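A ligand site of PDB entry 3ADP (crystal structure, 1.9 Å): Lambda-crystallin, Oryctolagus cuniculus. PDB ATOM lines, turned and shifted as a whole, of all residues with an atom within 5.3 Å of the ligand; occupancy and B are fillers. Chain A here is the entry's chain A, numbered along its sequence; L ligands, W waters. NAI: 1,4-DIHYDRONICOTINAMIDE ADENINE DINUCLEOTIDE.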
ATOM      1  N   VAL A  12      -7.566 -24.743  16.944  1.00  0.00           N
ATOM      2  CA  VAL A  12      -8.881 -24.358  17.448  1.00  0.00           C
ATOM      3  C   VAL A  12      -9.800 -24.261  16.229  1.00  0.00           C
ATOM      4  O   VAL A  12      -9.724 -23.305  15.455  1.00  0.00           O
ATOM      5  CB  VAL A  12      -8.835 -23.010  18.181  1.00  0.00           C
ATOM      6  CG1 VAL A  12     -10.249 -22.590  18.599  1.00  0.00           C
ATOM      7  CG2 VAL A  12      -7.940 -23.117  19.417  1.00  0.00           C
ATOM      8  N   GLY A  13     -10.656 -25.259  16.071  1.00  0.00           N
ATOM      9  CA  GLY A  13     -11.562 -25.299  14.935  1.00  0.00           C
ATOM     10  C   GLY A  13     -11.024 -26.320  13.943  1.00  0.00           C
ATOM     11  O   GLY A  13     -10.153 -26.002  13.130  1.00  0.00           O
ATOM     12  N   SER A  14     -11.523 -27.550  14.033  1.00  0.00           N
ATOM     13  CA  SER A  14     -11.058 -28.622  13.151  1.00  0.00           C
ATOM     14  C   SER A  14     -11.884 -28.733  11.874  1.00  0.00           C
ATOM     15  O   SER A  14     -12.414 -29.802  11.548  1.00  0.00           O
ATOM     16  CB  SER A  14     -11.070 -29.968  13.906  1.00  0.00           C
ATOM     17  OG  SER A  14     -12.380 -30.306  14.339  1.00  0.00           O
ATOM     18  N   GLY A  15     -11.991 -27.610  11.170  1.00  0.00           N
ATOM     19  CA  GLY A  15     -12.724 -27.565   9.918  1.00  0.00           C
ATOM     20  C   GLY A  15     -11.774 -27.772   8.753  1.00  0.00           C
ATOM     21  O   GLY A  15     -10.719 -28.387   8.905  1.00  0.00           O
ATOM     22  N   LEU A  16     -12.126 -27.243   7.586  1.00  0.00           N
ATOM     23  CA  LEU A  16     -11.287 -27.414   6.415  1.00  0.00           C
ATOM     24  C   LEU A  16      -9.833 -26.987   6.591  1.00  0.00           C
ATOM     25  O   LEU A  16      -8.919 -27.786   6.362  1.00  0.00           O
ATOM     26  CB  LEU A  16     -11.889 -26.682   5.207  1.00  0.00           C
ATOM     27  CG  LEU A  16     -13.288 -27.162   4.802  1.00  0.00           C
ATOM     28  CD1 LEU A  16     -13.714 -26.441   3.525  1.00  0.00           C
ATOM     29  CD2 LEU A  16     -13.276 -28.667   4.581  1.00  0.00           C
ATOM     30  N   VAL A  17      -9.604 -25.750   7.019  1.00  0.00           N
ATOM     31  CA  VAL A  17      -8.232 -25.287   7.185  1.00  0.00           C
ATOM     32  C   VAL A  17      -7.555 -25.900   8.419  1.00  0.00           C
ATOM     33  O   VAL A  17      -6.357 -26.162   8.411  1.00  0.00           O
ATOM     34  CB  VAL A  17      -8.161 -23.735   7.252  1.00  0.00           C
ATOM     35  CG1 VAL A  17      -8.518 -23.235   8.635  1.00  0.00           C
ATOM     36  CG2 VAL A  17      -6.762 -23.273   6.843  1.00  0.00           C
ATOM     37  N   GLY A  18      -8.339 -26.159   9.464  1.00  0.00           N
ATOM     38  CA  GLY A  18      -7.772 -26.774  10.657  1.00  0.00           C
ATOM     39  C   GLY A  18      -7.210 -28.154  10.359  1.00  0.00           C
ATOM     40  O   GLY A  18      -6.169 -28.552  10.893  1.00  0.00           O
ATOM     41  N   TYR A  35      -9.294 -29.102  18.732  1.00  0.00           N
ATOM     42  CA  TYR A  35     -10.342 -28.637  19.613  1.00  0.00           C
ATOM     43  C   TYR A  35     -11.433 -28.006  18.759  1.00  0.00           C
ATOM     44  O   TYR A  35     -11.141 -27.223  17.859  1.00  0.00           O
ATOM     45  CB  TYR A  35      -9.822 -27.599  20.605  1.00  0.00           C
ATOM     46  CG  TYR A  35     -10.929 -26.971  21.417  1.00  0.00           C
ATOM     47  CD1 TYR A  35     -11.499 -27.635  22.506  1.00  0.00           C
ATOM     48  CD2 TYR A  35     -11.459 -25.724  21.067  1.00  0.00           C
ATOM     49  CE1 TYR A  35     -12.568 -27.094  23.206  1.00  0.00           C
ATOM     50  CE2 TYR A  35     -12.527 -25.171  21.758  1.00  0.00           C
ATOM     51  CZ  TYR A  35     -13.076 -25.860  22.831  1.00  0.00           C
ATOM     52  OH  TYR A  35     -14.153 -25.309  23.502  1.00  0.00           O
ATOM     53  N   ASP A  36     -12.690 -28.329  19.056  1.00  0.00           N
ATOM     54  CA  ASP A  36     -13.801 -27.773  18.304  1.00  0.00           C
ATOM     55  C   ASP A  36     -15.046 -27.766  19.188  1.00  0.00           C
ATOM     56  O   ASP A  36     -15.197 -28.616  20.067  1.00  0.00           O
ATOM     57  CB  ASP A  36     -14.074 -28.608  17.043  1.00  0.00           C
ATOM     58  CG  ASP A  36     -14.806 -27.812  15.975  1.00  0.00           C
ATOM     59  OD1 ASP A  36     -15.991 -27.462  16.182  1.00  0.00           O
ATOM     60  OD2 ASP A  36     -14.191 -27.546  14.926  1.00  0.00           O
ATOM     61  N   ILE A  37     -15.942 -26.818  18.944  1.00  0.00           N
ATOM     62  CA  ILE A  37     -17.170 -26.704  19.720  1.00  0.00           C
ATOM     63  C   ILE A  37     -18.189 -27.752  19.292  1.00  0.00           C
ATOM     64  O   ILE A  37     -19.145 -28.040  20.003  1.00  0.00           O
ATOM     65  CB  ILE A  37     -17.783 -25.295  19.561  1.00  0.00           C
ATOM     66  CG1 ILE A  37     -18.928 -25.114  20.568  1.00  0.00           C
ATOM     67  CG2 ILE A  37     -18.296 -25.103  18.143  1.00  0.00           C
ATOM     68  CD1 ILE A  37     -18.454 -24.640  21.940  1.00  0.00           C
ATOM     69  N   GLU A  38     -17.983 -28.324  18.108  1.00  0.00           N
ATOM     70  CA  GLU A  38     -18.884 -29.326  17.563  1.00  0.00           C
ATOM     71  C   GLU A  38     -18.207 -30.689  17.477  1.00  0.00           C
ATOM     72  O   GLU A  38     -17.262 -30.877  16.706  1.00  0.00           O
ATOM     73  CB  GLU A  38     -19.366 -28.903  16.171  1.00  0.00           C
ATOM     74  CG  GLU A  38     -20.145 -29.968  15.416  1.00  0.00           C
ATOM     75  CD  GLU A  38     -21.340 -30.477  16.195  1.00  0.00           C
ATOM     76  OE1 GLU A  38     -22.169 -29.650  16.620  1.00  0.00           O
ATOM     77  OE2 GLU A  38     -21.450 -31.708  16.372  1.00  0.00           O
ATOM     78  N   GLN A  41     -17.398 -32.302  14.157  1.00  0.00           N
ATOM     79  CA  GLN A  41     -16.287 -31.737  13.396  1.00  0.00           C
ATOM     80  C   GLN A  41     -14.974 -32.395  13.783  1.00  0.00           C
ATOM     81  O   GLN A  41     -14.047 -32.481  12.965  1.00  0.00           O
ATOM     82  CB  GLN A  41     -16.212 -30.224  13.619  1.00  0.00           C
ATOM     83  CG  GLN A  41     -17.269 -29.407  12.869  1.00  0.00           C
ATOM     84  CD  GLN A  41     -17.209 -29.620  11.359  1.00  0.00           C
ATOM     85  OE1 GLN A  41     -17.902 -30.477  10.815  1.00  0.00           O
ATOM     86  NE2 GLN A  41     -16.363 -28.843  10.688  1.00  0.00           N
ATOM     87  N   GLU A  93      -5.693 -20.607  15.269  1.00  0.00           N
ATOM     88  CA  GLU A  93      -7.154 -20.455  15.285  1.00  0.00           C
ATOM     89  C   GLU A  93      -7.670 -20.665  13.871  1.00  0.00           C
ATOM     90  O   GLU A  93      -7.163 -20.071  12.918  1.00  0.00           O
ATOM     91  CB  GLU A  93      -7.527 -19.067  15.821  1.00  0.00           C
ATOM     92  CG  GLU A  93      -8.972 -18.664  15.593  1.00  0.00           C
ATOM     93  CD  GLU A  93      -9.156 -17.995  14.247  1.00  0.00           C
ATOM     94  OE1 GLU A  93      -8.397 -17.048  13.968  1.00  0.00           O
ATOM     95  OE2 GLU A  93     -10.057 -18.404  13.486  1.00  0.00           O
ATOM     96  N   CYS A  94      -8.690 -21.520  13.752  1.00  0.00           N
ATOM     97  CA  CYS A  94      -9.268 -21.853  12.460  1.00  0.00           C
ATOM     98  C   CYS A  94     -10.792 -21.870  12.469  1.00  0.00           C
ATOM     99  O   CYS A  94     -11.416 -22.778  11.921  1.00  0.00           O
ATOM    100  CB  CYS A  94      -8.748 -23.217  12.010  1.00  0.00           C
ATOM    101  SG  CYS A  94      -6.937 -23.359  12.045  1.00  0.00           S
ATOM    102  N   VAL A  95     -11.400 -20.874  13.113  1.00  0.00           N
ATOM    103  CA  VAL A  95     -12.858 -20.807  13.156  1.00  0.00           C
ATOM    104  C   VAL A  95     -13.328 -19.938  11.980  1.00  0.00           C
ATOM    105  O   VAL A  95     -12.511 -19.319  11.305  1.00  0.00           O
ATOM    106  CB  VAL A  95     -13.359 -20.228  14.511  1.00  0.00           C
ATOM    107  CG1 VAL A  95     -12.767 -21.044  15.663  1.00  0.00           C
ATOM    108  CG2 VAL A  95     -12.966 -18.750  14.646  1.00  0.00           C
ATOM    109  N   PRO A  96     -14.646 -19.901  11.711  1.00  0.00           N
ATOM    110  CA  PRO A  96     -15.166 -19.105  10.591  1.00  0.00           C
ATOM    111  C   PRO A  96     -14.669 -17.656  10.540  1.00  0.00           C
ATOM    112  O   PRO A  96     -14.308 -17.064  11.565  1.00  0.00           O
ATOM    113  CB  PRO A  96     -16.677 -19.192  10.791  1.00  0.00           C
ATOM    114  CG  PRO A  96     -16.848 -20.570  11.361  1.00  0.00           C
ATOM    115  CD  PRO A  96     -15.728 -20.621  12.394  1.00  0.00           C
ATOM    116  N   GLU A  97     -14.645 -17.095   9.334  1.00  0.00           N
ATOM    117  CA  GLU A  97     -14.201 -15.727   9.082  1.00  0.00           C
ATOM    118  C   GLU A  97     -15.264 -14.739   9.577  1.00  0.00           C
ATOM    119  O   GLU A  97     -15.979 -14.121   8.784  1.00  0.00           O
ATOM    120  CB  GLU A  97     -13.957 -15.529   7.585  1.00  0.00           C
ATOM    121  CG  GLU A  97     -13.371 -14.169   7.192  1.00  0.00           C
ATOM    122  CD  GLU A  97     -11.894 -14.029   7.526  1.00  0.00           C
ATOM    123  OE1 GLU A  97     -11.321 -14.929   8.173  1.00  0.00           O
ATOM    124  OE2 GLU A  97     -11.301 -12.994   7.143  1.00  0.00           O
ATOM    125  N   LEU A 101     -16.686 -13.507  16.388  1.00  0.00           N
ATOM    126  CA  LEU A 101     -16.310 -14.832  16.845  1.00  0.00           C
ATOM    127  C   LEU A 101     -14.808 -14.965  17.117  1.00  0.00           C
ATOM    128  O   LEU A 101     -14.421 -15.495  18.157  1.00  0.00           O
ATOM    129  CB  LEU A 101     -16.736 -15.890  15.826  1.00  0.00           C
ATOM    130  CG  LEU A 101     -16.389 -17.337  16.200  1.00  0.00           C
ATOM    131  CD1 LEU A 101     -17.043 -17.684  17.526  1.00  0.00           C
ATOM    132  CD2 LEU A 101     -16.860 -18.279  15.095  1.00  0.00           C
ATOM    133  N   LYS A 102     -13.971 -14.505  16.195  1.00  0.00           N
ATOM    134  CA  LYS A 102     -12.537 -14.616  16.412  1.00  0.00           C
ATOM    135  C   LYS A 102     -12.124 -13.828  17.645  1.00  0.00           C
ATOM    136  O   LYS A 102     -11.281 -14.274  18.429  1.00  0.00           O
ATOM    137  CB  LYS A 102     -11.750 -14.134  15.182  1.00  0.00           C
ATOM    138  CG  LYS A 102     -11.925 -15.022  13.950  1.00  0.00           C
ATOM    139  CD  LYS A 102     -10.816 -14.761  12.923  1.00  0.00           C
ATOM    140  CE  LYS A 102     -11.100 -15.458  11.594  1.00  0.00           C
ATOM    141  NZ  LYS A 102     -11.350 -16.925  11.753  1.00  0.00           N
ATOM    142  N   LYS A 104     -13.858 -13.291  20.281  1.00  0.00           N
ATOM    143  CA  LYS A 104     -14.236 -14.065  21.450  1.00  0.00           C
ATOM    144  C   LYS A 104     -13.248 -15.193  21.693  1.00  0.00           C
ATOM    145  O   LYS A 104     -12.857 -15.453  22.828  1.00  0.00           O
ATOM    146  CB  LYS A 104     -15.651 -14.647  21.281  1.00  0.00           C
ATOM    147  CG  LYS A 104     -16.093 -15.456  22.495  1.00  0.00           C
ATOM    148  CD  LYS A 104     -17.517 -15.980  22.350  1.00  0.00           C
ATOM    149  CE  LYS A 104     -17.619 -17.042  21.270  1.00  0.00           C
ATOM    150  NZ  LYS A 104     -18.977 -17.645  21.236  1.00  0.00           N
ATOM    151  N   ILE A 105     -12.821 -15.856  20.627  1.00  0.00           N
ATOM    152  CA  ILE A 105     -11.866 -16.958  20.754  1.00  0.00           C
ATOM    153  C   ILE A 105     -10.553 -16.497  21.357  1.00  0.00           C
ATOM    154  O   ILE A 105     -10.030 -17.113  22.292  1.00  0.00           O
ATOM    155  CB  ILE A 105     -11.558 -17.601  19.369  1.00  0.00           C
ATOM    156  CG1 ILE A 105     -12.804 -18.296  18.833  1.00  0.00           C
ATOM    157  CG2 ILE A 105     -10.406 -18.594  19.504  1.00  0.00           C
ATOM    158  CD1 ILE A 105     -13.342 -19.394  19.729  1.00  0.00           C
ATOM    159  N   GLN A 108     -10.863 -15.642  24.986  1.00  0.00           N
ATOM    160  CA  GLN A 108     -10.928 -16.851  25.807  1.00  0.00           C
ATOM    161  C   GLN A 108      -9.538 -17.440  25.990  1.00  0.00           C
ATOM    162  O   GLN A 108      -9.188 -17.911  27.072  1.00  0.00           O
ATOM    163  CB  GLN A 108     -11.884 -17.877  25.177  1.00  0.00           C
ATOM    164  CG  GLN A 108     -13.309 -17.345  25.041  1.00  0.00           C
ATOM    165  CD  GLN A 108     -14.260 -18.314  24.368  1.00  0.00           C
ATOM    166  OE1 GLN A 108     -13.938 -18.932  23.367  1.00  0.00           O
ATOM    167  NE2 GLN A 108     -15.466 -18.423  24.917  1.00  0.00           N
ATOM    168  N   SER A 122      -5.848 -17.819  11.350  1.00  0.00           N
ATOM    169  CA  SER A 122      -5.775 -18.190   9.930  1.00  0.00           C
ATOM    170  C   SER A 122      -6.539 -17.204   9.046  1.00  0.00           C
ATOM    171  O   SER A 122      -6.626 -17.355   7.829  1.00  0.00           O
ATOM    172  CB  SER A 122      -6.378 -19.586   9.732  1.00  0.00           C
ATOM    173  OG  SER A 122      -5.704 -20.557  10.543  1.00  0.00           O
ATOM    174  N   SER A 123      -7.145 -16.187   9.698  1.00  0.00           N
ATOM    175  CA  SER A 123      -8.001 -15.210   8.999  1.00  0.00           C
ATOM    176  C   SER A 123      -7.524 -14.844   7.591  1.00  0.00           C
ATOM    177  O   SER A 123      -6.358 -14.513   7.357  1.00  0.00           O
ATOM    178  CB  SER A 123      -8.088 -13.944   9.829  1.00  0.00           C
ATOM    179  OG  SER A 123      -9.095 -13.089   9.264  1.00  0.00           O
ATOM    180  N   SER A 124      -8.471 -14.857   6.662  1.00  0.00           N
ATOM    181  CA  SER A 124      -8.190 -14.526   5.267  1.00  0.00           C
ATOM    182  C   SER A 124      -8.132 -13.033   4.993  1.00  0.00           C
ATOM    183  O   SER A 124      -7.466 -12.608   4.052  1.00  0.00           O
ATOM    184  CB  SER A 124      -9.250 -15.149   4.356  1.00  0.00           C
ATOM    185  OG  SER A 124      -9.267 -16.566   4.468  1.00  0.00           O
ATOM    186  N   HIS A 145      -1.791 -16.464   7.757  1.00  0.00           N
ATOM    187  CA  HIS A 145      -2.748 -16.801   6.712  1.00  0.00           C
ATOM    188  C   HIS A 145      -2.216 -17.734   5.628  1.00  0.00           C
ATOM    189  O   HIS A 145      -1.339 -17.353   4.850  1.00  0.00           O
ATOM    190  CB  HIS A 145      -3.264 -15.513   6.081  1.00  0.00           C
ATOM    191  CG  HIS A 145      -4.103 -15.738   4.863  1.00  0.00           C
ATOM    192  ND1 HIS A 145      -3.768 -15.218   3.627  1.00  0.00           N
ATOM    193  CD2 HIS A 145      -5.258 -16.423   4.685  1.00  0.00           C
ATOM    194  CE1 HIS A 145      -4.683 -15.592   2.739  1.00  0.00           C
ATOM    195  NE2 HIS A 145      -5.590 -16.323   3.355  1.00  0.00           N
ATOM    196  N   PRO A 146      -2.732 -18.972   5.577  1.00  0.00           N
ATOM    197  CA  PRO A 146      -2.319 -19.961   4.582  1.00  0.00           C
ATOM    198  C   PRO A 146      -3.112 -19.754   3.296  1.00  0.00           C
ATOM    199  O   PRO A 146      -3.996 -18.897   3.236  1.00  0.00           O
ATOM    200  CB  PRO A 146      -2.661 -21.277   5.263  1.00  0.00           C
ATOM    201  CG  PRO A 146      -3.941 -20.933   5.968  1.00  0.00           C
ATOM    202  CD  PRO A 146      -3.652 -19.559   6.567  1.00  0.00           C
ATOM    203  N   VAL A 147      -2.796 -20.541   2.266  1.00  0.00           N
ATOM    204  CA  VAL A 147      -3.472 -20.433   0.985  1.00  0.00           C
ATOM    205  C   VAL A 147      -4.059 -21.793   0.607  1.00  0.00           C
ATOM    206  O   VAL A 147      -3.353 -22.789   0.563  1.00  0.00           O
ATOM    207  CB  VAL A 147      -2.493 -19.999  -0.122  1.00  0.00           C
ATOM    208  CG1 VAL A 147      -3.222 -19.842  -1.453  1.00  0.00           C
ATOM    209  CG2 VAL A 147      -1.818 -18.706   0.286  1.00  0.00           C
ATOM    210  N   ASN A 148      -5.354 -21.822   0.334  1.00  0.00           N
ATOM    211  CA  ASN A 148      -5.999 -23.075  -0.028  1.00  0.00           C
ATOM    212  C   ASN A 148      -5.578 -23.564  -1.413  1.00  0.00           C
ATOM    213  O   ASN A 148      -5.587 -22.794  -2.391  1.00  0.00           O
ATOM    214  CB  ASN A 148      -7.521 -22.925   0.032  1.00  0.00           C
ATOM    215  CG  ASN A 148      -8.239 -24.177  -0.419  1.00  0.00           C
ATOM    216  OD1 ASN A 148      -8.563 -24.347  -1.596  1.00  0.00           O
ATOM    217  ND2 ASN A 148      -8.480 -25.092   0.515  1.00  0.00           N
ATOM    218  N   PRO A 150      -3.630 -25.502   1.508  1.00  0.00           N
ATOM    219  CA  PRO A 150      -2.365 -25.372   2.244  1.00  0.00           C
ATOM    220  C   PRO A 150      -1.351 -26.503   2.127  1.00  0.00           C
ATOM    221  O   PRO A 150      -0.138 -26.268   2.213  1.00  0.00           O
ATOM    222  CB  PRO A 150      -2.818 -25.161   3.689  1.00  0.00           C
ATOM    223  CG  PRO A 150      -4.166 -24.507   3.528  1.00  0.00           C
ATOM    224  CD  PRO A 150      -4.772 -25.324   2.415  1.00  0.00           C
HETATM  225  PA  NAI L   1     -14.893 -24.125   8.483  1.00  0.00           P
HETATM  226  O1A NAI L   1     -16.282 -23.683   8.648  1.00  0.00           O
HETATM  227  O2A NAI L   1     -14.794 -25.392   7.737  1.00  0.00           O
HETATM  228  O5B NAI L   1     -14.142 -24.436   9.859  1.00  0.00           O
HETATM  229  C5B NAI L   1     -14.393 -23.658  11.058  1.00  0.00           C
HETATM  230  C4B NAI L   1     -14.440 -24.596  12.250  1.00  0.00           C
HETATM  231  O4B NAI L   1     -14.672 -23.724  13.390  1.00  0.00           O
HETATM  232  C3B NAI L   1     -15.633 -25.581  12.297  1.00  0.00           C
HETATM  233  O3B NAI L   1     -15.152 -26.936  12.403  1.00  0.00           O
HETATM  234  C2B NAI L   1     -16.444 -25.098  13.516  1.00  0.00           C
HETATM  235  O2B NAI L   1     -17.138 -26.153  14.213  1.00  0.00           O
HETATM  236  C1B NAI L   1     -15.369 -24.445  14.347  1.00  0.00           C
HETATM  237  N9A NAI L   1     -15.892 -23.514  15.336  1.00  0.00           N
HETATM  238  C8A NAI L   1     -16.922 -22.598  15.240  1.00  0.00           C
HETATM  239  N7A NAI L   1     -17.133 -21.877  16.376  1.00  0.00           N
HETATM  240  C5A NAI L   1     -16.164 -22.391  17.241  1.00  0.00           C
HETATM  241  C6A NAI L   1     -15.837 -22.063  18.619  1.00  0.00           C
HETATM  242  N6A NAI L   1     -16.479 -21.135  19.332  1.00  0.00           N
HETATM  243  N1A NAI L   1     -14.781 -22.774  19.184  1.00  0.00           N
HETATM  244  C2A NAI L   1     -14.114 -23.744  18.439  1.00  0.00           C
HETATM  245  N3A NAI L   1     -14.346 -24.101  17.183  1.00  0.00           N
HETATM  246  C4A NAI L   1     -15.384 -23.394  16.629  1.00  0.00           C
HETATM  247  O3  NAI L   1     -14.073 -23.015   7.740  1.00  0.00           O
HETATM  248  PN  NAI L   1     -12.550 -22.929   7.246  1.00  0.00           P
HETATM  249  O1N NAI L   1     -12.714 -22.922   5.755  1.00  0.00           O
HETATM  250  O2N NAI L   1     -11.831 -24.117   7.684  1.00  0.00           O
HETATM  251  O5D NAI L   1     -11.860 -21.533   7.581  1.00  0.00           O
HETATM  252  C5D NAI L   1     -11.451 -21.195   8.918  1.00  0.00           C
HETATM  253  C4D NAI L   1     -10.716 -19.855   8.839  1.00  0.00           C
HETATM  254  O4D NAI L   1      -9.533 -20.065   7.991  1.00  0.00           O
HETATM  255  C3D NAI L   1     -11.480 -18.673   8.229  1.00  0.00           C
HETATM  256  O3D NAI L   1     -11.194 -17.431   8.913  1.00  0.00           O
HETATM  257  C2D NAI L   1     -10.986 -18.679   6.773  1.00  0.00           C
HETATM  258  O2D NAI L   1     -11.160 -17.362   6.180  1.00  0.00           O
HETATM  259  C1D NAI L   1      -9.540 -19.110   6.943  1.00  0.00           C
HETATM  260  N1N NAI L   1      -8.914 -19.675   5.706  1.00  0.00           N
HETATM  261  C2N NAI L   1      -9.357 -20.957   5.366  1.00  0.00           C
HETATM  262  C3N NAI L   1      -8.744 -21.545   4.253  1.00  0.00           C
HETATM  263  C7N NAI L   1      -9.174 -22.917   3.731  1.00  0.00           C
HETATM  264  O7N NAI L   1      -8.371 -23.583   3.083  1.00  0.00           O
HETATM  265  N7N NAI L   1     -10.433 -23.354   3.956  1.00  0.00           N
HETATM  266  C4N NAI L   1      -7.610 -20.903   3.583  1.00  0.00           C
HETATM  267  C5N NAI L   1      -7.047 -19.802   4.283  1.00  0.00           C
HETATM  268  C6N NAI L   1      -7.626 -19.149   5.364  1.00  0.00           C
HETATM  269  O   HOH W   1     -19.754 -25.273  14.292  1.00  0.00           O
HETATM  270  O   HOH W   2     -15.669 -28.016   8.018  1.00  0.00           O
HETATM  271  O   HOH W   3     -19.587 -20.590  16.778  1.00  0.00           O
HETATM  272  O   HOH W   4     -19.128 -19.833  19.397  1.00  0.00           O
HETATM  273  O   HOH W   5      -7.994 -26.427   3.685  1.00  0.00           O
HETATM  274  O   HOH W   6     -19.092 -22.753  12.704  1.00  0.00           O
HETATM  275  O   HOH W   7     -16.411 -25.825   5.185  1.00  0.00           O
HETATM  276  O   HOH W   8     -15.083 -23.630   4.164  1.00  0.00           O
HETATM  277  O   HOH W   9     -11.053 -25.150  10.229  1.00  0.00           O
HETATM  278  O   HOH W  10     -13.260 -17.577   4.762  1.00  0.00           O
HETATM  279  O   HOH W  11     -15.809 -20.586  22.419  1.00  0.00           O
HETATM  280  O   HOH W  12     -16.938 -21.092   7.684  1.00  0.00           O
HETATM  281  O   HOH W  13     -13.870 -20.389   5.076  1.00  0.00           O
HETATM  282  O   HOH W  14     -18.434 -24.081  10.193  1.00  0.00           O
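Water W2 bridges an oxygen (O2A) of the ligand (2.8 Å) and the side-chain amide nitrogen of Gln 41 (2.9 Å). Water W9 lies within hydrogen-bond range of the backbone NH (N) of Gly 15 (2.8 Å), an oxygen (O2N) of the ligand (2.9 Å), the backbone carbonyl oxygen (O) of Cys 94 (2.9 Å), the backbone NH (N) of Gly 18 (3.0 Å) and the backbone carbonyl oxygen (O) of Gly 13 (3.2 Å). Water W5 lies within hydrogen-bond range of O7N of the ligand (2.9 Å), O of Leu 16 (3.1 Å) and ND2 of Asn 148 (3.5 Å). Water W4 lies within hydrogen-bond range of the side-chain amino group of Lys 104 (2.9 Å) and a nitrogen (N6A) of the ligand (3.0 Å). Water W11 bridges OE1 of Gln 108 (2.7 Å) and N6A of the ligand (3.2 Å).
O3D of the ligand sits close to N of Glu 97 (3.5 Å). The side-chain carboxylate (OE1) of Glu 97 is in hydrogen-bond range of an oxygen (O3D) of the ligand, 2.6 Å away. The side-chain carboxylate (OD1) of Asp 36 is in hydrogen-bond range of an oxygen (O2B) of the ligand (2.6 Å). An oxygen (O2D) of the ligand is in hydrogen-bond range of the side-chain hydroxyl (OG) of Ser 124. An oxygen (O3B) of the ligand is in hydrogen-bond range of the side-chain amide nitrogen (NE2) of Gln 41 (2.8 Å). The backbone NH (N) of Val 17 is in hydrogen-bond range of an oxygen (O2N) of the ligand, at 2.8 Å. The side-chain amino group (NZ) of Lys 102 is in hydrogen-bond range of an oxygen (O3D) of the ligand, 2.9 Å away. An oxygen (O7N) of the ligand lies within hydrogen-bond range of the side-chain amide nitrogen (ND2) of Asn 148 (3.0 Å). An oxygen (O3D) of the ligand lies close to the backbone carbonyl oxygen of Val 95 (3.3 Å). N of Leu 16 sits at hydrogen-bond distance from O2N of the ligand, 3.1 Å away. The backbone NH of Gly 15 is in hydrogen-bond range of an oxygen (O3B) of the ligand.
The side-chain carboxylate (OE1) of Glu 97 is in hydrogen-bond range of the backbone NH (N) of Ser 124 (3.2 Å). The side-chain carboxylate (OE2) of Glu 97 lies within hydrogen-bond range of the side-chain hydroxyl (OG) of Ser 123 (3.1 Å). The backbone NH (N) of Ser 14 is in hydrogen-bond range of the side-chain carboxylate (OD2) of Asp 36, 2.8 Å away. OD1 of Asp 36 is in hydrogen-bond range of N of Glu 38 (2.9 Å). The backbone carbonyl oxygen (O) of Gln 41 sits at hydrogen-bond distance from the side-chain hydroxyl (OG) of Ser 14 (3.1 Å). The side-chain carboxylate of Glu 93 is in salt-bridge range of the side-chain amino group of Lys 102, at 2.6 Å. O of Glu 93 is in hydrogen-bond range of OG of Ser 122 (2.8 Å). N of Cys 94 lies within hydrogen-bond range of O of Val 12 (2.7 Å).
Gly 13 touches the ligand. Ser 14 touches the ligand (C to O3B, 3.8 Å). Tyr 35 touches the ligand (CE2 to C2A, 3.9 Å). Ile 37 touches the ligand. Cys 94 touches the ligand. Pro 96 touches the ligand. CD2 of Leu 101 touches N7A of the ligand, 3.8 Å away. CD1 of Ile 105 touches N6A of the ligand, at 3.6 Å. Ser 122 touches the ligand (O to C6N, 3.2 Å). Ser 123 touches the ligand (CA to O3D, 3.9 Å). CD2 of His 145 touches C6N of the ligand, 3.7 Å away. O of Pro 146 touches C5N of the ligand (3.4 Å). Hydrophobic or aromatic side chains within 4 Å of the ligand: Leu 16, Val 17, Tyr 35, Ile 37, Val 95, Pro 96, Leu 101, Ile 105, His 145 and Pro 146. 22 residues have an atom within 4 Å of the ligand: Gly 13, Ser 14, Gly 15, Leu 16, Val 17, Tyr 35, Asp 36, Ile 37, Gln 41, Cys 94, Val 95, Pro 96, Glu 97, Leu 101, Lys 102, Ile 105, Ser 122, Ser 123, Ser 124, His 145, Pro 146 and Asn 148.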
